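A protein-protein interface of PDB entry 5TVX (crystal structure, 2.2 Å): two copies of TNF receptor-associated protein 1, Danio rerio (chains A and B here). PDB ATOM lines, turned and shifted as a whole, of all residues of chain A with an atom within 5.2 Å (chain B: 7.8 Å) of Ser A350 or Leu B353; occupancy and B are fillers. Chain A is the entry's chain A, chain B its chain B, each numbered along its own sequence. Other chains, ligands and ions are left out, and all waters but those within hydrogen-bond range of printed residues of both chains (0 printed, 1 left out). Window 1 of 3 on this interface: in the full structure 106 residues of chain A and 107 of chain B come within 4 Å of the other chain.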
ATOM      1  N   LEU A  54      11.728  -4.448 -14.758  1.00  0.00           N
ATOM      2  CA  LEU A  54      10.943  -3.220 -14.712  1.00  0.00           C
ATOM      3  C   LEU A  54      11.196  -2.307 -15.900  1.00  0.00           C
ATOM      4  O   LEU A  54      10.254  -1.737 -16.455  1.00  0.00           O
ATOM      5  CB  LEU A  54      11.255  -2.446 -13.424  1.00  0.00           C
ATOM      6  CG  LEU A  54      10.126  -2.127 -12.483  1.00  0.00           C
ATOM      7  CD1 LEU A  54       9.275  -3.366 -12.413  1.00  0.00           C
ATOM      8  CD2 LEU A  54      10.700  -1.756 -11.113  1.00  0.00           C
ATOM      9  N   TYR A  55      12.453  -2.162 -16.297  1.00  0.00           N
ATOM     10  CA  TYR A  55      12.920  -1.104 -17.176  1.00  0.00           C
ATOM     11  C   TYR A  55      13.306  -1.682 -18.520  1.00  0.00           C
ATOM     12  O   TYR A  55      13.605  -2.870 -18.651  1.00  0.00           O
ATOM     13  CB  TYR A  55      14.138  -0.410 -16.575  1.00  0.00           C
ATOM     14  CG  TYR A  55      13.923  -0.001 -15.160  1.00  0.00           C
ATOM     15  CD1 TYR A  55      13.159   1.137 -14.849  1.00  0.00           C
ATOM     16  CD2 TYR A  55      14.464  -0.742 -14.124  1.00  0.00           C
ATOM     17  CE1 TYR A  55      12.956   1.514 -13.548  1.00  0.00           C
ATOM     18  CE2 TYR A  55      14.269  -0.358 -12.808  1.00  0.00           C
ATOM     19  CZ  TYR A  55      13.499   0.759 -12.525  1.00  0.00           C
ATOM     20  OH  TYR A  55      13.288   1.133 -11.216  1.00  0.00           O
ATOM     21  N   SER A  56      13.357  -0.823 -19.516  1.00  0.00           N
ATOM     22  CA  SER A  56      13.667  -1.353 -20.827  1.00  0.00           C
ATOM     23  C   SER A  56      15.163  -1.382 -21.107  1.00  0.00           C
ATOM     24  O   SER A  56      15.558  -1.895 -22.157  1.00  0.00           O
ATOM     25  CB  SER A  56      12.932  -0.548 -21.898  1.00  0.00           C
ATOM     26  OG  SER A  56      13.371   0.789 -21.894  1.00  0.00           O
ATOM     27  N   ARG A  63      20.339   6.469 -13.687  1.00  0.00           N
ATOM     28  CA  ARG A  63      19.247   7.416 -13.499  1.00  0.00           C
ATOM     29  C   ARG A  63      18.670   7.317 -12.094  1.00  0.00           C
ATOM     30  O   ARG A  63      18.461   8.342 -11.424  1.00  0.00           O
ATOM     31  CB  ARG A  63      18.143   7.168 -14.525  1.00  0.00           C
ATOM     32  CG  ARG A  63      17.038   8.245 -14.495  1.00  0.00           C
ATOM     33  CD  ARG A  63      15.784   7.807 -15.247  1.00  0.00           C
ATOM     34  NE  ARG A  63      15.090   6.742 -14.542  1.00  0.00           N
ATOM     35  CZ  ARG A  63      14.326   5.824 -15.132  1.00  0.00           C
ATOM     36  NH1 ARG A  63      14.163   5.820 -16.451  1.00  0.00           N
ATOM     37  NH2 ARG A  63      13.742   4.887 -14.406  1.00  0.00           N
ATOM     38  N   ASN A 348       4.191   5.598 -15.023  1.00  0.00           N
ATOM     39  CA  ASN A 348       4.361   4.160 -14.894  1.00  0.00           C
ATOM     40  C   ASN A 348       5.491   3.845 -13.907  1.00  0.00           C
ATOM     41  O   ASN A 348       6.451   4.612 -13.777  1.00  0.00           O
ATOM     42  CB  ASN A 348       4.666   3.616 -16.280  1.00  0.00           C
ATOM     43  CG  ASN A 348       4.749   2.162 -16.311  1.00  0.00           C
ATOM     44  OD1 ASN A 348       5.828   1.605 -16.228  1.00  0.00           O
ATOM     45  ND2 ASN A 348       3.599   1.505 -16.425  1.00  0.00           N
ATOM     46  N   LEU A 349       5.369   2.703 -13.205  1.00  0.00           N
ATOM     47  CA  LEU A 349       6.444   2.223 -12.325  1.00  0.00           C
ATOM     48  C   LEU A 349       7.828   2.311 -12.963  1.00  0.00           C
ATOM     49  O   LEU A 349       8.814   2.561 -12.269  1.00  0.00           O
ATOM     50  CB  LEU A 349       6.213   0.768 -11.912  1.00  0.00           C
ATOM     51  CG  LEU A 349       7.113   0.204 -10.794  1.00  0.00           C
ATOM     52  CD1 LEU A 349       6.974   1.045  -9.522  1.00  0.00           C
ATOM     53  CD2 LEU A 349       6.824  -1.262 -10.481  1.00  0.00           C
ATOM     54  N   SER A 350       7.929   2.091 -14.270  1.00  0.00           N
ATOM     55  CA  SER A 350       9.223   2.135 -14.935  1.00  0.00           C
ATOM     56  C   SER A 350       9.790   3.546 -15.060  1.00  0.00           C
ATOM     57  O   SER A 350      10.970   3.680 -15.389  1.00  0.00           O
ATOM     58  CB  SER A 350       9.112   1.539 -16.333  1.00  0.00           C
ATOM     59  OG  SER A 350       8.356   2.409 -17.167  1.00  0.00           O
ATOM     60  N   ARG A 351       8.979   4.587 -14.854  1.00  0.00           N
ATOM     61  CA  ARG A 351       9.401   5.967 -15.111  1.00  0.00           C
ATOM     62  C   ARG A 351       9.793   6.190 -16.569  1.00  0.00           C
ATOM     63  O   ARG A 351      10.653   7.013 -16.877  1.00  0.00           O
ATOM     64  CB  ARG A 351      10.553   6.368 -14.195  1.00  0.00           C
ATOM     65  CG  ARG A 351      10.205   6.225 -12.759  1.00  0.00           C
ATOM     66  CD  ARG A 351      11.424   6.411 -11.897  1.00  0.00           C
ATOM     67  NE  ARG A 351      11.006   6.566 -10.517  1.00  0.00           N
ATOM     68  CZ  ARG A 351      10.385   7.645 -10.054  1.00  0.00           C
ATOM     69  NH1 ARG A 351      10.127   8.664 -10.880  1.00  0.00           N
ATOM     70  NH2 ARG A 351      10.033   7.697  -8.769  1.00  0.00           N
ATOM     71  N   GLU A 352       9.199   5.441 -17.480  1.00  0.00           N
ATOM     72  CA  GLU A 352       9.470   5.628 -18.892  1.00  0.00           C
ATOM     73  C   GLU A 352       8.190   5.720 -19.694  1.00  0.00           C
ATOM     74  O   GLU A 352       8.256   5.772 -20.924  1.00  0.00           O
ATOM     75  CB  GLU A 352      10.328   4.484 -19.443  1.00  0.00           C
ATOM     76  CG  GLU A 352      11.191   3.844 -18.381  1.00  0.00           C
ATOM     77  CD  GLU A 352      12.210   2.886 -18.937  1.00  0.00           C
ATOM     78  OE1 GLU A 352      13.366   3.313 -19.122  1.00  0.00           O
ATOM     79  OE2 GLU A 352      11.854   1.716 -19.200  1.00  0.00           O
ATOM     80  N   LEU A 353       7.036   5.710 -19.027  1.00  0.00           N
ATOM     81  CA  LEU A 353       5.725   5.744 -19.653  1.00  0.00           C
ATOM     82  C   LEU A 353       4.782   6.531 -18.760  1.00  0.00           C
ATOM     83  O   LEU A 353       4.966   6.607 -17.544  1.00  0.00           O
ATOM     84  CB  LEU A 353       5.147   4.333 -19.846  1.00  0.00           C
ATOM     85  CG  LEU A 353       5.889   3.362 -20.743  1.00  0.00           C
ATOM     86  CD1 LEU A 353       5.260   1.959 -20.685  1.00  0.00           C
ATOM     87  CD2 LEU A 353       5.866   3.907 -22.157  1.00  0.00           C
ATOM     88  N   SER B  53      -0.170   1.547 -11.204  1.00  0.00           N
ATOM     89  CA  SER B  53       1.118   2.046 -11.655  1.00  0.00           C
ATOM     90  C   SER B  53       1.862   1.085 -12.566  1.00  0.00           C
ATOM     91  O   SER B  53       2.838   1.496 -13.209  1.00  0.00           O
ATOM     92  CB  SER B  53       2.004   2.402 -10.450  1.00  0.00           C
ATOM     93  OG  SER B  53       1.626   3.649  -9.864  1.00  0.00           O
ATOM     94  N   LEU B  54       1.417  -0.162 -12.674  1.00  0.00           N
ATOM     95  CA  LEU B  54       2.210  -1.159 -13.383  1.00  0.00           C
ATOM     96  C   LEU B  54       1.977  -1.119 -14.896  1.00  0.00           C
ATOM     97  O   LEU B  54       2.937  -1.027 -15.671  1.00  0.00           O
ATOM     98  CB  LEU B  54       1.910  -2.539 -12.812  1.00  0.00           C
ATOM     99  CG  LEU B  54       2.818  -3.627 -13.353  1.00  0.00           C
ATOM    100  CD1 LEU B  54       4.283  -3.186 -13.204  1.00  0.00           C
ATOM    101  CD2 LEU B  54       2.526  -4.918 -12.614  1.00  0.00           C
ATOM    102  N   LEU B 314       4.655  -7.122 -33.096  1.00  0.00           N
ATOM    103  CA  LEU B 314       5.669  -7.852 -32.352  1.00  0.00           C
ATOM    104  C   LEU B 314       4.989  -8.711 -31.297  1.00  0.00           C
ATOM    105  O   LEU B 314       4.108  -8.227 -30.576  1.00  0.00           O
ATOM    106  CB  LEU B 314       6.664  -6.882 -31.702  1.00  0.00           C
ATOM    107  CG  LEU B 314       7.894  -7.428 -30.977  1.00  0.00           C
ATOM    108  CD1 LEU B 314       8.827  -8.182 -31.930  1.00  0.00           C
ATOM    109  CD2 LEU B 314       8.644  -6.283 -30.345  1.00  0.00           C
ATOM    110  N   LEU B 320       0.817  -9.897 -27.552  1.00  0.00           N
ATOM    111  CA  LEU B 320       1.360  -8.740 -28.238  1.00  0.00           C
ATOM    112  C   LEU B 320       2.403  -7.968 -27.409  1.00  0.00           C
ATOM    113  O   LEU B 320       2.414  -7.976 -26.179  1.00  0.00           O
ATOM    114  CB  LEU B 320       0.177  -7.855 -28.609  1.00  0.00           C
ATOM    115  CG  LEU B 320       0.233  -6.622 -29.480  1.00  0.00           C
ATOM    116  CD1 LEU B 320       0.550  -7.054 -30.867  1.00  0.00           C
ATOM    117  CD2 LEU B 320      -1.134  -5.943 -29.396  1.00  0.00           C
ATOM    118  N   ILE B 321       3.301  -7.290 -28.114  1.00  0.00           N
ATOM    119  CA  ILE B 321       4.248  -6.369 -27.503  1.00  0.00           C
ATOM    120  C   ILE B 321       4.142  -5.019 -28.207  1.00  0.00           C
ATOM    121  O   ILE B 321       4.048  -4.950 -29.439  1.00  0.00           O
ATOM    122  CB  ILE B 321       5.700  -6.889 -27.576  1.00  0.00           C
ATOM    123  CG1 ILE B 321       5.766  -8.400 -27.327  1.00  0.00           C
ATOM    124  CG2 ILE B 321       6.580  -6.143 -26.565  1.00  0.00           C
ATOM    125  CD1 ILE B 321       5.468  -8.796 -25.905  1.00  0.00           C
ATOM    126  N   GLN B 322       4.168  -3.944 -27.426  1.00  0.00           N
ATOM    127  CA  GLN B 322       4.298  -2.603 -27.991  1.00  0.00           C
ATOM    128  C   GLN B 322       5.781  -2.201 -28.087  1.00  0.00           C
ATOM    129  O   GLN B 322       6.255  -1.737 -29.132  1.00  0.00           O
ATOM    130  CB  GLN B 322       3.528  -1.574 -27.142  1.00  0.00           C
ATOM    131  CG  GLN B 322       2.286  -2.118 -26.421  1.00  0.00           C
ATOM    132  CD  GLN B 322       1.172  -2.556 -27.371  1.00  0.00           C
ATOM    133  OE1 GLN B 322       1.196  -3.666 -27.909  1.00  0.00           O
ATOM    134  NE2 GLN B 322       0.188  -1.683 -27.573  1.00  0.00           N
ATOM    135  N   ILE B 345      13.559 -11.754 -26.979  1.00  0.00           N
ATOM    136  CA  ILE B 345      13.156 -10.432 -26.520  1.00  0.00           C
ATOM    137  C   ILE B 345      12.665 -10.554 -25.085  1.00  0.00           C
ATOM    138  O   ILE B 345      11.548 -11.037 -24.865  1.00  0.00           O
ATOM    139  CB  ILE B 345      12.064  -9.851 -27.426  1.00  0.00           C
ATOM    140  CG1 ILE B 345      12.548  -9.873 -28.877  1.00  0.00           C
ATOM    141  CG2 ILE B 345      11.691  -8.459 -26.959  1.00  0.00           C
ATOM    142  CD1 ILE B 345      11.567  -9.287 -29.852  1.00  0.00           C
ATOM    143  N   PRO B 346      13.439 -10.158 -24.080  1.00  0.00           N
ATOM    144  CA  PRO B 346      12.903 -10.187 -22.720  1.00  0.00           C
ATOM    145  C   PRO B 346      11.828  -9.125 -22.606  1.00  0.00           C
ATOM    146  O   PRO B 346      11.885  -8.085 -23.265  1.00  0.00           O
ATOM    147  CB  PRO B 346      14.118  -9.865 -21.835  1.00  0.00           C
ATOM    148  CG  PRO B 346      15.304  -9.741 -22.782  1.00  0.00           C
ATOM    149  CD  PRO B 346      14.717  -9.434 -24.131  1.00  0.00           C
ATOM    150  N   LEU B 347      10.818  -9.414 -21.804  1.00  0.00           N
ATOM    151  CA  LEU B 347       9.726  -8.480 -21.582  1.00  0.00           C
ATOM    152  C   LEU B 347       9.795  -7.961 -20.168  1.00  0.00           C
ATOM    153  O   LEU B 347      10.070  -8.718 -19.233  1.00  0.00           O
ATOM    154  CB  LEU B 347       8.354  -9.116 -21.782  1.00  0.00           C
ATOM    155  CG  LEU B 347       8.208  -9.932 -23.036  1.00  0.00           C
ATOM    156  CD1 LEU B 347       6.800 -10.511 -23.053  1.00  0.00           C
ATOM    157  CD2 LEU B 347       8.495  -8.993 -24.193  1.00  0.00           C
ATOM    158  N   ASN B 348       9.523  -6.670 -20.030  1.00  0.00           N
ATOM    159  CA  ASN B 348       9.368  -6.086 -18.721  1.00  0.00           C
ATOM    160  C   ASN B 348       8.098  -6.624 -18.060  1.00  0.00           C
ATOM    161  O   ASN B 348       7.266  -7.294 -18.684  1.00  0.00           O
ATOM    162  CB  ASN B 348       9.313  -4.566 -18.819  1.00  0.00           C
ATOM    163  CG  ASN B 348       7.974  -4.076 -19.350  1.00  0.00           C
ATOM    164  OD1 ASN B 348       7.353  -4.720 -20.207  1.00  0.00           O
ATOM    165  ND2 ASN B 348       7.509  -2.947 -18.825  1.00  0.00           N
ATOM    166  N   LEU B 349       7.953  -6.285 -16.778  1.00  0.00           N
ATOM    167  CA  LEU B 349       6.858  -6.777 -15.953  1.00  0.00           C
ATOM    168  C   LEU B 349       5.497  -6.510 -16.561  1.00  0.00           C
ATOM    169  O   LEU B 349       4.546  -7.245 -16.281  1.00  0.00           O
ATOM    170  CB  LEU B 349       6.941  -6.117 -14.595  1.00  0.00           C
ATOM    171  CG  LEU B 349       5.979  -6.542 -13.518  1.00  0.00           C
ATOM    172  CD1 LEU B 349       6.011  -8.047 -13.366  1.00  0.00           C
ATOM    173  CD2 LEU B 349       6.423  -5.847 -12.267  1.00  0.00           C
ATOM    174  N   SER B 350       5.391  -5.486 -17.395  1.00  0.00           N
ATOM    175  CA  SER B 350       4.119  -5.017 -17.907  1.00  0.00           C
ATOM    176  C   SER B 350       3.764  -5.623 -19.243  1.00  0.00           C
ATOM    177  O   SER B 350       2.603  -5.520 -19.655  1.00  0.00           O
ATOM    178  CB  SER B 350       4.145  -3.494 -18.046  1.00  0.00           C
ATOM    179  OG  SER B 350       5.134  -3.119 -18.990  1.00  0.00           O
ATOM    180  N   ARG B 351       4.737  -6.230 -19.931  1.00  0.00           N
ATOM    181  CA  ARG B 351       4.531  -6.869 -21.233  1.00  0.00           C
ATOM    182  C   ARG B 351       4.201  -5.833 -22.294  1.00  0.00           C
ATOM    183  O   ARG B 351       3.369  -6.065 -23.167  1.00  0.00           O
ATOM    184  CB  ARG B 351       3.444  -7.950 -21.194  1.00  0.00           C
ATOM    185  CG  ARG B 351       3.726  -9.131 -20.284  1.00  0.00           C
ATOM    186  CD  ARG B 351       2.450  -9.954 -20.076  1.00  0.00           C
ATOM    187  NE  ARG B 351       2.586 -10.946 -19.013  1.00  0.00           N
ATOM    188  CZ  ARG B 351       3.207 -12.112 -19.163  1.00  0.00           C
ATOM    189  NH1 ARG B 351       3.754 -12.424 -20.335  1.00  0.00           N
ATOM    190  NH2 ARG B 351       3.287 -12.958 -18.139  1.00  0.00           N
ATOM    191  N   GLU B 352       4.843  -4.673 -22.206  1.00  0.00           N
ATOM    192  CA  GLU B 352       4.757  -3.688 -23.283  1.00  0.00           C
ATOM    193  C   GLU B 352       6.089  -3.052 -23.631  1.00  0.00           C
ATOM    194  O   GLU B 352       6.222  -2.503 -24.730  1.00  0.00           O
ATOM    195  CB  GLU B 352       3.746  -2.580 -22.940  1.00  0.00           C
ATOM    196  CG  GLU B 352       3.435  -2.400 -21.464  1.00  0.00           C
ATOM    197  CD  GLU B 352       2.651  -1.102 -21.179  1.00  0.00           C
ATOM    198  OE1 GLU B 352       2.532  -0.271 -22.109  1.00  0.00           O
ATOM    199  OE2 GLU B 352       2.169  -0.918 -20.030  1.00  0.00           O
ATOM    200  N   LEU B 353       7.081  -3.117 -22.763  1.00  0.00           N
ATOM    201  CA  LEU B 353       8.432  -2.695 -23.080  1.00  0.00           C
ATOM    202  C   LEU B 353       9.267  -3.920 -23.437  1.00  0.00           C
ATOM    203  O   LEU B 353       9.096  -4.997 -22.859  1.00  0.00           O
ATOM    204  CB  LEU B 353       9.061  -1.941 -21.896  1.00  0.00           C
ATOM    205  CG  LEU B 353       8.638  -0.509 -21.508  1.00  0.00           C
ATOM    206  CD1 LEU B 353       9.074  -0.156 -20.067  1.00  0.00           C
ATOM    207  CD2 LEU B 353       9.188   0.525 -22.498  1.00  0.00           C
ATOM    208  N   LEU B 354      10.156  -3.754 -24.405  1.00  0.00           N
ATOM    209  CA  LEU B 354      11.187  -4.727 -24.741  1.00  0.00           C
ATOM    210  C   LEU B 354      12.530  -4.235 -24.196  1.00  0.00           C
ATOM    211  O   LEU B 354      12.803  -3.031 -24.175  1.00  0.00           O
ATOM    212  CB  LEU B 354      11.241  -4.952 -26.258  1.00  0.00           C
ATOM    213  CG  LEU B 354      11.462  -3.809 -27.272  1.00  0.00           C
ATOM    214  CD1 LEU B 354      11.430  -4.381 -28.678  1.00  0.00           C
ATOM    215  CD2 LEU B 354      10.465  -2.634 -27.179  1.00  0.00           C
ATOM    216  N   GLN B 355      13.373  -5.173 -23.748  1.00  0.00           N
ATOM    217  CA  GLN B 355      14.334  -4.869 -22.691  1.00  0.00           C
ATOM    218  C   GLN B 355      15.803  -4.752 -23.107  1.00  0.00           C
ATOM    219  O   GLN B 355      16.632  -4.421 -22.249  1.00  0.00           O
ATOM    220  CB  GLN B 355      14.216  -5.908 -21.568  1.00  0.00           C
ATOM    221  CG  GLN B 355      13.423  -5.424 -20.368  1.00  0.00           C
ATOM    222  CD  GLN B 355      13.618  -6.298 -19.135  1.00  0.00           C
ATOM    223  OE1 GLN B 355      13.741  -7.517 -19.237  1.00  0.00           O
ATOM    224  NE2 GLN B 355      13.643  -5.672 -17.960  1.00  0.00           N
ATOM    225  N   GLU B 356      16.177  -5.006 -24.361  1.00  0.00           N
ATOM    226  CA  GLU B 356      17.582  -4.832 -24.756  1.00  0.00           C
ATOM    227  C   GLU B 356      17.641  -4.207 -26.146  1.00  0.00           C
ATOM    228  O   GLU B 356      17.269  -4.843 -27.136  1.00  0.00           O
ATOM    229  CB  GLU B 356      18.357  -6.154 -24.716  1.00  0.00           C
ATOM    230  CG  GLU B 356      18.249  -6.929 -23.395  1.00  0.00           C
ATOM    231  CD  GLU B 356      19.460  -7.810 -23.096  1.00  0.00           C
ATOM    232  OE1 GLU B 356      20.043  -7.663 -21.999  1.00  0.00           O
ATOM    233  OE2 GLU B 356      19.829  -8.645 -23.947  1.00  0.00           O
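Printed residues of chain B that touch a printed residue of chain A: Ser B53, Leu B54, Asn B348, Leu B349, Glu B352, Leu B353, Leu B354, Gln B355 and Glu B356.
Hydrophobic or aromatic side chains of chain B within 4 Å of the printed part of chain A: Leu B349 and Leu B353.
Along chain A the printed residues that touch a printed residue of chain B span positions 54 to 353.
OD1 of Asn B348 sits at hydrogen-bond distance from N of Glu B352 (3.2 Å).
The side-chain amide oxygen (OD1) of Asn B348 sits at hydrogen-bond distance from the backbone NH (N) of Leu B353 (3.0 Å).
The backbone NH (N) of Ser A56 lies within hydrogen-bond range of the side-chain carboxylate (OE2) of Glu A352 (3.0 Å).
The side-chain amide oxygen (OD1) of Asn A348 lies within hydrogen-bond range of the side-chain hydroxyl (OG) of Ser A350 (2.8 Å).
N of Asn A348 sits at hydrogen-bond distance from O of Leu A353 (2.8 Å).
The side-chain hydroxyl of Ser A350 sits close to the backbone NH of Glu A352 (3.2 Å).
The side-chain amide nitrogen (ND2) of Asn A348 lies within hydrogen-bond range of the backbone carbonyl oxygen (O) of Ser B53, at 3.3 Å.
O of Ser B53 lies within hydrogen-bond range of N of Leu A349 (2.8 Å).
The backbone carbonyl oxygen of Leu B54 lies within hydrogen-bond range of the side-chain amide nitrogen of Asn A348, 2.7 Å away.
O of Tyr A55 is in hydrogen-bond range of NE2 of Gln B355.
The backbone carbonyl oxygen (O) of Gln B355 lies close to the backbone carbonyl oxygen (O) of Ser A56.
Ser A350 touches one residue of chain B.
Leu B353 touches just these residues of chain A: Ser A56 (3.9 Å), Ser A350 (3.9 Å) and Glu A352 (3.5 Å).
Of the printed residues of chain A, Ser B53 touches Asn A348 and Leu A349.
Printed residues of chain A within 4 Å of Glu B356: Ser A56.
Printed residues of chain B within 4 Å of Glu A352: Leu B353.
Printed residues of chain B within 4 Å of Leu A349: Ser B53.
Printed residues of chain B within 4 Å of Leu A353: Glu B352.
Leu A54 touches Asn B348 (O to CB, 3.8 Å).
Leu B349 touches Leu A54.
N of Leu A54 touches NE2 of Gln B355, 3.9 Å away.
CB of Ser A56 touches CD2 of Leu B353, at 3.9 Å.
O of Leu B354 touches CB of Ser A56 (3.4 Å).
O of Ser A56 touches N of Glu B356 (3.9 Å).
Ser A350 touches Leu B353.
Leu B353 touches Glu A352 (CD1 to OE2, 3.5 Å).
Leu A353 touches Glu B352.
Leu A54 touches Asn B348, and with the chains exchanged Asn A348 touches Leu B54.
Leu A54 touches Leu B349, but with the chains exchanged Leu A349 does not touch Leu B54 (4.2 Å).
Ser A350 touches Leu B353, but with the chains exchanged Leu A353 does not touch Ser B350 (5.4 Å).
Glu A352 touches Leu B353, and with the chains exchanged Leu A353 touches Glu B352.
Positions printed for both chains: 54, 348, 349, 350, 351, 352 and 353.
Of the 14 pairs that touch across the chains among the printed residues, 4 have their exchanged pair printed and touching as well.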
